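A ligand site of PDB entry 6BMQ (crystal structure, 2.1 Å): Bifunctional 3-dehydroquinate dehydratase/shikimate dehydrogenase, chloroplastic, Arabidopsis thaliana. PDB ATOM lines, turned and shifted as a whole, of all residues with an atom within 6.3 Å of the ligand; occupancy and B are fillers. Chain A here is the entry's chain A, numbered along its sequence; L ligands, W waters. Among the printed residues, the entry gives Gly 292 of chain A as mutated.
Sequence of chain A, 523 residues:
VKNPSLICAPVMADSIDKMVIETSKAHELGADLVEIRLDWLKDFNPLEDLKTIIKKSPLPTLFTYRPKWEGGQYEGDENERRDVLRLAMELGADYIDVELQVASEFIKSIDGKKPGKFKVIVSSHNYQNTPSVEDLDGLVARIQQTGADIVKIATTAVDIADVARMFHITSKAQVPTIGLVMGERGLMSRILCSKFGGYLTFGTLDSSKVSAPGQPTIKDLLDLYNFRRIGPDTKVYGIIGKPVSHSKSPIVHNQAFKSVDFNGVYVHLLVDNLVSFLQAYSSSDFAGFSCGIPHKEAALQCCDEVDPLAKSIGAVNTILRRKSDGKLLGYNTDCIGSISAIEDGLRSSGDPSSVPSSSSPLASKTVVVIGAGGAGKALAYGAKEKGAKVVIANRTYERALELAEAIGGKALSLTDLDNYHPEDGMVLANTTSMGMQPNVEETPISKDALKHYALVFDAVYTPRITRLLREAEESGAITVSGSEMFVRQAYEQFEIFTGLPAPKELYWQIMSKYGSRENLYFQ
The side-chain hydroxyl of Ser 249 sits at hydrogen-bond distance from an oxygen (O5) of the ligand (2.7 Å). ND2 of Asn 317 lies within hydrogen-bond range of O3 of the ligand (2.9 Å). An oxygen (O3) of the ligand lies within hydrogen-bond range of the side-chain carboxylate (OD1) of Asp 334 (2.7 Å). O3 of the ligand sits at hydrogen-bond distance from NZ of Lys 296 (2.9 Å). The side-chain amide nitrogen (NE2) of Gln 493 is in hydrogen-bond range of an oxygen (O4) of the ligand. OH of Tyr 461 sits at hydrogen-bond distance from O6 of the ligand (2.5 Å). OG of Ser 247 lies within hydrogen-bond range of O5 of the ligand (2.5 Å).
The backbone NH (N) of Ile 239 lies close to the side-chain hydroxyl (OH) of Tyr 266, 3.4 Å away. NE2 of Gln 493 sits at hydrogen-bond distance from O of Asn 317. The side-chain carboxylate of Asp 334 is in hydrogen-bond range of the side-chain amide nitrogen of Asn 317, at 3.3 Å. The side-chain amide nitrogen (NE2) of Gln 489 is in hydrogen-bond range of the backbone carbonyl oxygen (O) of Phe 486 (3.0 Å). The side-chain amide nitrogen of Gln 493 sits close to the side-chain amide oxygen of Gln 489, at 3.4 Å. The side-chain hydroxyl (OG1) of Thr 333 lies within hydrogen-bond range of the backbone carbonyl oxygen (O) of Gln 489, at 3.0 Å. NZ of Lys 296 is in salt-bridge range of OD2 of Asp 334, 2.6 Å away. The side-chain hydroxyl (OH) of Tyr 461 sits at hydrogen-bond distance from the backbone NH (N) of Lys 248 (3.0 Å).
CD1 of Ile 239 touches C6 of the ligand, 3.6 Å away. Ser 290 touches the ligand. O of Cys 291 touches O4 of the ligand, 3.5 Å away. Gly 292 touches the ligand (CA to O1, 3.95 Å). Phe 486 touches the ligand. Gln 489 touches the ligand. Hydrophobic or aromatic side chains within 4 Å of the ligand: Ile 239, Tyr 461 and Phe 486. The nearest printed residue that does not touch the ligand is His 246 (4.1 Å).
Water W4 lies within hydrogen-bond range of NE2 of His 246 (2.7 Å) and O1 of the ligand (2.8 Å). Water W2 bridges an oxygen (O6) of the ligand (3.0 Å) and a ring nitrogen (NE2) of His 246 (3.4 Å). Water W1 bridges N of Ile 293 (2.8 Å) and O2 of the ligand (3.1 Å).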
ATOM      1  N   ILE A 239       7.290  -0.206  19.001  1.00  0.00           N
ATOM      2  CA  ILE A 239       5.911  -0.560  19.359  1.00  0.00           C
ATOM      3  C   ILE A 239       5.174  -1.127  18.121  1.00  0.00           C
ATOM      4  O   ILE A 239       4.925  -0.412  17.139  1.00  0.00           O
ATOM      5  CB  ILE A 239       5.157   0.651  19.969  1.00  0.00           C
ATOM      6  CG1 ILE A 239       3.648   0.384  20.041  1.00  0.00           C
ATOM      7  CG2 ILE A 239       5.422   1.938  19.186  1.00  0.00           C
ATOM      8  CD1 ILE A 239       3.275  -0.759  20.910  1.00  0.00           C
ATOM      9  N   HIS A 246      -0.188   7.256  17.494  1.00  0.00           N
ATOM     10  CA  HIS A 246      -0.493   7.972  18.720  1.00  0.00           C
ATOM     11  C   HIS A 246       0.500   7.654  19.841  1.00  0.00           C
ATOM     12  O   HIS A 246       0.578   8.391  20.827  1.00  0.00           O
ATOM     13  CB  HIS A 246      -1.872   7.576  19.206  1.00  0.00           C
ATOM     14  CG  HIS A 246      -1.939   6.133  19.559  1.00  0.00           C
ATOM     15  ND1 HIS A 246      -2.030   5.140  18.600  1.00  0.00           N
ATOM     16  CD2 HIS A 246      -1.824   5.499  20.752  1.00  0.00           C
ATOM     17  CE1 HIS A 246      -2.022   3.960  19.192  1.00  0.00           C
ATOM     18  NE2 HIS A 246      -1.886   4.148  20.494  1.00  0.00           N
ATOM     19  N   SER A 247       1.237   6.558  19.679  1.00  0.00           N
ATOM     20  CA  SER A 247       2.013   6.005  20.798  1.00  0.00           C
ATOM     21  C   SER A 247       3.147   6.912  21.252  1.00  0.00           C
ATOM     22  O   SER A 247       3.916   7.438  20.444  1.00  0.00           O
ATOM     23  CB  SER A 247       2.589   4.629  20.426  1.00  0.00           C
ATOM     24  OG  SER A 247       3.412   4.129  21.482  1.00  0.00           O
ATOM     25  N   LYS A 248       3.230   7.104  22.565  1.00  0.00           N
ATOM     26  CA  LYS A 248       4.348   7.834  23.140  1.00  0.00           C
ATOM     27  C   LYS A 248       5.423   6.879  23.666  1.00  0.00           C
ATOM     28  O   LYS A 248       6.344   7.316  24.350  1.00  0.00           O
ATOM     29  CB  LYS A 248       3.853   8.763  24.249  1.00  0.00           C
ATOM     30  CG  LYS A 248       2.969   9.852  23.706  1.00  0.00           C
ATOM     31  CD  LYS A 248       2.566  10.879  24.753  1.00  0.00           C
ATOM     32  CE  LYS A 248       1.724  11.969  24.097  1.00  0.00           C
ATOM     33  NZ  LYS A 248       1.247  12.959  25.099  1.00  0.00           N
ATOM     34  N   SER A 249       5.319   5.583  23.351  1.00  0.00           N
ATOM     35  CA  SER A 249       6.364   4.621  23.733  1.00  0.00           C
ATOM     36  C   SER A 249       7.742   5.031  23.172  1.00  0.00           C
ATOM     37  O   SER A 249       8.748   4.973  23.884  1.00  0.00           O
ATOM     38  CB  SER A 249       5.999   3.204  23.299  1.00  0.00           C
ATOM     39  OG  SER A 249       5.041   2.646  24.177  1.00  0.00           O
ATOM     40  N   PRO A 250       7.798   5.447  21.891  1.00  0.00           N
ATOM     41  CA  PRO A 250       9.116   5.925  21.452  1.00  0.00           C
ATOM     42  C   PRO A 250       9.607   7.168  22.219  1.00  0.00           C
ATOM     43  O   PRO A 250      10.802   7.305  22.406  1.00  0.00           O
ATOM     44  CB  PRO A 250       8.902   6.239  19.973  1.00  0.00           C
ATOM     45  CG  PRO A 250       7.803   5.333  19.566  1.00  0.00           C
ATOM     46  CD  PRO A 250       6.870   5.288  20.748  1.00  0.00           C
ATOM     47  N   TYR A 266      14.226   3.213  19.711  1.00  0.00           N
ATOM     48  CA  TYR A 266      12.849   2.727  19.733  1.00  0.00           C
ATOM     49  C   TYR A 266      12.028   3.487  18.689  1.00  0.00           C
ATOM     50  O   TYR A 266      12.063   4.723  18.653  1.00  0.00           O
ATOM     51  CB  TYR A 266      12.274   2.903  21.138  1.00  0.00           C
ATOM     52  CG  TYR A 266      10.977   2.198  21.426  1.00  0.00           C
ATOM     53  CD1 TYR A 266       9.769   2.685  20.947  1.00  0.00           C
ATOM     54  CD2 TYR A 266      10.955   1.063  22.226  1.00  0.00           C
ATOM     55  CE1 TYR A 266       8.581   2.060  21.233  1.00  0.00           C
ATOM     56  CE2 TYR A 266       9.766   0.424  22.521  1.00  0.00           C
ATOM     57  CZ  TYR A 266       8.596   0.933  22.017  1.00  0.00           C
ATOM     58  OH  TYR A 266       7.426   0.312  22.332  1.00  0.00           O
ATOM     59  N   SER A 290       7.443  -3.755  21.959  1.00  0.00           N
ATOM     60  CA  SER A 290       6.211  -3.635  22.702  1.00  0.00           C
ATOM     61  C   SER A 290       5.097  -4.020  21.733  1.00  0.00           C
ATOM     62  O   SER A 290       5.204  -3.752  20.516  1.00  0.00           O
ATOM     63  CB  SER A 290       6.011  -2.206  23.269  1.00  0.00           C
ATOM     64  OG  SER A 290       7.173  -1.719  23.951  1.00  0.00           O
ATOM     65  N   CYS A 291       4.049  -4.664  22.229  1.00  0.00           N
ATOM     66  CA  CYS A 291       2.899  -5.049  21.398  1.00  0.00           C
ATOM     67  C   CYS A 291       1.638  -4.315  21.798  1.00  0.00           C
ATOM     68  O   CYS A 291       1.179  -4.456  22.932  1.00  0.00           O
ATOM     69  CB  CYS A 291       2.637  -6.557  21.456  1.00  0.00           C
ATOM     70  SG  CYS A 291       3.996  -7.545  20.847  1.00  0.00           S
ATOM     71  N   GLY A 292       1.082  -3.527  20.890  1.00  0.00           N
ATOM     72  CA  GLY A 292      -0.190  -2.869  21.138  1.00  0.00           C
ATOM     73  C   GLY A 292      -1.312  -3.515  20.351  1.00  0.00           C
ATOM     74  O   GLY A 292      -1.113  -4.518  19.666  1.00  0.00           O
ATOM     75  N   ILE A 293      -2.505  -2.935  20.474  1.00  0.00           N
ATOM     76  CA  ILE A 293      -3.660  -3.285  19.654  1.00  0.00           C
ATOM     77  C   ILE A 293      -3.270  -3.255  18.177  1.00  0.00           C
ATOM     78  O   ILE A 293      -2.637  -2.300  17.740  1.00  0.00           O
ATOM     79  CB  ILE A 293      -4.828  -2.293  19.952  1.00  0.00           C
ATOM     80  CG1 ILE A 293      -5.354  -2.512  21.366  1.00  0.00           C
ATOM     81  CG2 ILE A 293      -5.972  -2.440  18.936  1.00  0.00           C
ATOM     82  CD1 ILE A 293      -6.315  -1.461  21.843  1.00  0.00           C
ATOM     83  N   LYS A 296      -1.702  -8.018  20.706  1.00  0.00           N
ATOM     84  CA  LYS A 296      -1.279  -8.499  22.020  1.00  0.00           C
ATOM     85  C   LYS A 296      -1.599  -9.968  22.209  1.00  0.00           C
ATOM     86  O   LYS A 296      -0.736 -10.774  22.517  1.00  0.00           O
ATOM     87  CB  LYS A 296      -1.931  -7.684  23.129  1.00  0.00           C
ATOM     88  CG  LYS A 296      -1.450  -6.259  23.221  1.00  0.00           C
ATOM     89  CD  LYS A 296      -2.151  -5.526  24.336  1.00  0.00           C
ATOM     90  CE  LYS A 296      -1.588  -4.120  24.450  1.00  0.00           C
ATOM     91  NZ  LYS A 296      -1.828  -3.549  25.778  1.00  0.00           N
ATOM     92  N   ASN A 317       2.235  -8.379  25.771  1.00  0.00           N
ATOM     93  CA  ASN A 317       2.465  -6.974  25.353  1.00  0.00           C
ATOM     94  C   ASN A 317       3.959  -6.624  25.238  1.00  0.00           C
ATOM     95  O   ASN A 317       4.298  -5.543  24.764  1.00  0.00           O
ATOM     96  CB  ASN A 317       1.751  -5.999  26.309  1.00  0.00           C
ATOM     97  CG  ASN A 317       2.579  -5.651  27.535  1.00  0.00           C
ATOM     98  OD1 ASN A 317       3.296  -6.487  28.083  1.00  0.00           O
ATOM     99  ND2 ASN A 317       2.483  -4.397  27.968  1.00  0.00           N
ATOM    100  N   THR A 318       4.847  -7.555  25.622  1.00  0.00           N
ATOM    101  CA  THR A 318       6.302  -7.313  25.504  1.00  0.00           C
ATOM    102  C   THR A 318       7.037  -8.527  24.940  1.00  0.00           C
ATOM    103  O   THR A 318       6.900  -9.652  25.442  1.00  0.00           O
ATOM    104  CB  THR A 318       6.936  -6.947  26.878  1.00  0.00           C
ATOM    105  OG1 THR A 318       6.047  -6.112  27.618  1.00  0.00           O
ATOM    106  CG2 THR A 318       8.282  -6.231  26.688  1.00  0.00           C
ATOM    107  N   THR A 333       3.314  -6.828  30.826  1.00  0.00           N
ATOM    108  CA  THR A 333       3.492  -5.787  31.814  1.00  0.00           C
ATOM    109  C   THR A 333       2.203  -4.967  31.970  1.00  0.00           C
ATOM    110  O   THR A 333       2.154  -4.012  32.747  1.00  0.00           O
ATOM    111  CB  THR A 333       4.669  -4.840  31.452  1.00  0.00           C
ATOM    112  OG1 THR A 333       4.310  -4.048  30.322  1.00  0.00           O
ATOM    113  CG2 THR A 333       5.922  -5.640  31.119  1.00  0.00           C
ATOM    114  N   ASP A 334       1.170  -5.356  31.232  1.00  0.00           N
ATOM    115  CA  ASP A 334      -0.133  -4.676  31.360  1.00  0.00           C
ATOM    116  C   ASP A 334      -0.786  -4.957  32.716  1.00  0.00           C
ATOM    117  O   ASP A 334      -1.430  -4.078  33.290  1.00  0.00           O
ATOM    118  CB  ASP A 334      -1.094  -5.087  30.236  1.00  0.00           C
ATOM    119  CG  ASP A 334      -0.844  -4.349  28.912  1.00  0.00           C
ATOM    120  OD1 ASP A 334      -0.418  -3.160  28.939  1.00  0.00           O
ATOM    121  OD2 ASP A 334      -1.095  -4.957  27.842  1.00  0.00           O
ATOM    122  N   ALA A 375      -5.511  -6.097  26.770  1.00  0.00           N
ATOM    123  CA  ALA A 375      -5.496  -5.270  27.966  1.00  0.00           C
ATOM    124  C   ALA A 375      -6.610  -5.666  28.922  1.00  0.00           C
ATOM    125  O   ALA A 375      -6.438  -5.608  30.153  1.00  0.00           O
ATOM    126  CB  ALA A 375      -5.619  -3.795  27.601  1.00  0.00           C
ATOM    127  N   ALA A 459      -7.454   3.226  30.142  1.00  0.00           N
ATOM    128  CA  ALA A 459      -6.125   2.910  29.597  1.00  0.00           C
ATOM    129  C   ALA A 459      -5.663   3.883  28.501  1.00  0.00           C
ATOM    130  O   ALA A 459      -4.468   4.010  28.242  1.00  0.00           O
ATOM    131  CB  ALA A 459      -6.105   1.487  29.042  1.00  0.00           C
ATOM    132  N   TYR A 461      -4.363   7.002  26.978  1.00  0.00           N
ATOM    133  CA  TYR A 461      -3.622   8.145  27.494  1.00  0.00           C
ATOM    134  C   TYR A 461      -3.438   9.218  26.409  1.00  0.00           C
ATOM    135  O   TYR A 461      -2.780  10.218  26.627  1.00  0.00           O
ATOM    136  CB  TYR A 461      -2.259   7.698  28.084  1.00  0.00           C
ATOM    137  CG  TYR A 461      -1.313   7.119  27.053  1.00  0.00           C
ATOM    138  CD1 TYR A 461      -1.378   5.773  26.707  1.00  0.00           C
ATOM    139  CD2 TYR A 461      -0.356   7.909  26.422  1.00  0.00           C
ATOM    140  CE1 TYR A 461      -0.533   5.230  25.745  1.00  0.00           C
ATOM    141  CE2 TYR A 461       0.499   7.383  25.465  1.00  0.00           C
ATOM    142  CZ  TYR A 461       0.403   6.053  25.130  1.00  0.00           C
ATOM    143  OH  TYR A 461       1.246   5.531  24.179  1.00  0.00           O
ATOM    144  N   MET A 485      -1.146   4.046  34.268  1.00  0.00           N
ATOM    145  CA  MET A 485      -0.896   2.708  33.740  1.00  0.00           C
ATOM    146  C   MET A 485       0.292   2.692  32.759  1.00  0.00           C
ATOM    147  O   MET A 485       1.136   1.801  32.811  1.00  0.00           O
ATOM    148  CB  MET A 485      -2.143   2.152  33.049  1.00  0.00           C
ATOM    149  CG  MET A 485      -1.983   0.765  32.392  1.00  0.00           C
ATOM    150  SD  MET A 485      -1.175   0.673  30.755  1.00  0.00           S
ATOM    151  CE  MET A 485      -2.141   1.829  29.759  1.00  0.00           C
ATOM    152  N   PHE A 486       0.318   3.668  31.849  1.00  0.00           N
ATOM    153  CA  PHE A 486       1.286   3.664  30.755  1.00  0.00           C
ATOM    154  C   PHE A 486       2.724   3.695  31.264  1.00  0.00           C
ATOM    155  O   PHE A 486       3.571   2.932  30.818  1.00  0.00           O
ATOM    156  CB  PHE A 486       1.059   4.860  29.812  1.00  0.00           C
ATOM    157  CG  PHE A 486       2.094   4.957  28.732  1.00  0.00           C
ATOM    158  CD1 PHE A 486       2.113   4.036  27.684  1.00  0.00           C
ATOM    159  CD2 PHE A 486       3.065   5.942  28.765  1.00  0.00           C
ATOM    160  CE1 PHE A 486       3.066   4.109  26.677  1.00  0.00           C
ATOM    161  CE2 PHE A 486       4.023   6.023  27.760  1.00  0.00           C
ATOM    162  CZ  PHE A 486       4.025   5.099  26.716  1.00  0.00           C
ATOM    163  N   GLN A 489       3.712   0.287  33.074  1.00  0.00           N
ATOM    164  CA  GLN A 489       3.976  -0.870  32.229  1.00  0.00           C
ATOM    165  C   GLN A 489       5.233  -0.617  31.408  1.00  0.00           C
ATOM    166  O   GLN A 489       5.885  -1.551  30.952  1.00  0.00           O
ATOM    167  CB  GLN A 489       2.782  -1.206  31.329  1.00  0.00           C
ATOM    168  CG  GLN A 489       2.422  -0.140  30.286  1.00  0.00           C
ATOM    169  CD  GLN A 489       3.344  -0.162  29.073  1.00  0.00           C
ATOM    170  OE1 GLN A 489       3.881  -1.214  28.701  1.00  0.00           O
ATOM    171  NE2 GLN A 489       3.555   0.999  28.475  1.00  0.00           N
ATOM    172  N   GLN A 493       8.916  -2.604  30.868  1.00  0.00           N
ATOM    173  CA  GLN A 493       9.376  -3.056  29.555  1.00  0.00           C
ATOM    174  C   GLN A 493      10.848  -2.696  29.377  1.00  0.00           C
ATOM    175  O   GLN A 493      11.620  -3.462  28.779  1.00  0.00           O
ATOM    176  CB  GLN A 493       8.531  -2.447  28.423  1.00  0.00           C
ATOM    177  CG  GLN A 493       7.121  -2.990  28.350  1.00  0.00           C
ATOM    178  CD  GLN A 493       6.376  -2.584  27.069  1.00  0.00           C
ATOM    179  OE1 GLN A 493       6.674  -1.556  26.464  1.00  0.00           O
ATOM    180  NE2 GLN A 493       5.422  -3.416  26.653  1.00  0.00           N
HETATM  181  C1  LIG L   1       1.017   0.930  24.213  1.00  0.00           C
HETATM  182  O1  LIG L   1       0.053   0.375  23.380  1.00  0.00           O
HETATM  183  C2  LIG L   1       0.386   1.080  25.581  1.00  0.00           C
HETATM  184  O2  LIG L   1      -1.040  -0.741  25.233  1.00  0.00           O
HETATM  185  C3  LIG L   1      -0.086  -0.274  26.130  1.00  0.00           C
HETATM  186  O3  LIG L   1       0.743  -2.481  26.644  1.00  0.00           O
HETATM  187  C4  LIG L   1       1.173  -1.215  26.212  1.00  0.00           C
HETATM  188  O4  LIG L   1       2.971  -2.123  24.869  1.00  0.00           O
HETATM  189  C5  LIG L   1       1.796  -1.352  24.787  1.00  0.00           C
HETATM  190  O5  LIG L   1       2.563   2.508  23.221  1.00  0.00           O
HETATM  191  C6  LIG L   1       2.239   0.039  24.283  1.00  0.00           C
HETATM  192  O6  LIG L   1       0.520   3.192  23.636  1.00  0.00           O
HETATM  193  C7  LIG L   1       1.455   2.335  23.643  1.00  0.00           C
HETATM  194  O   HOH W   1      -2.638  -1.122  22.603  1.00  0.00           O
HETATM  195  O   HOH W   2      -2.467   3.214  23.763  1.00  0.00           O
HETATM  196  O   HOH W   3      -3.480  -0.168  26.984  1.00  0.00           O
HETATM  197  O   HOH W   4      -1.198   1.637  21.152  1.00  0.00           O
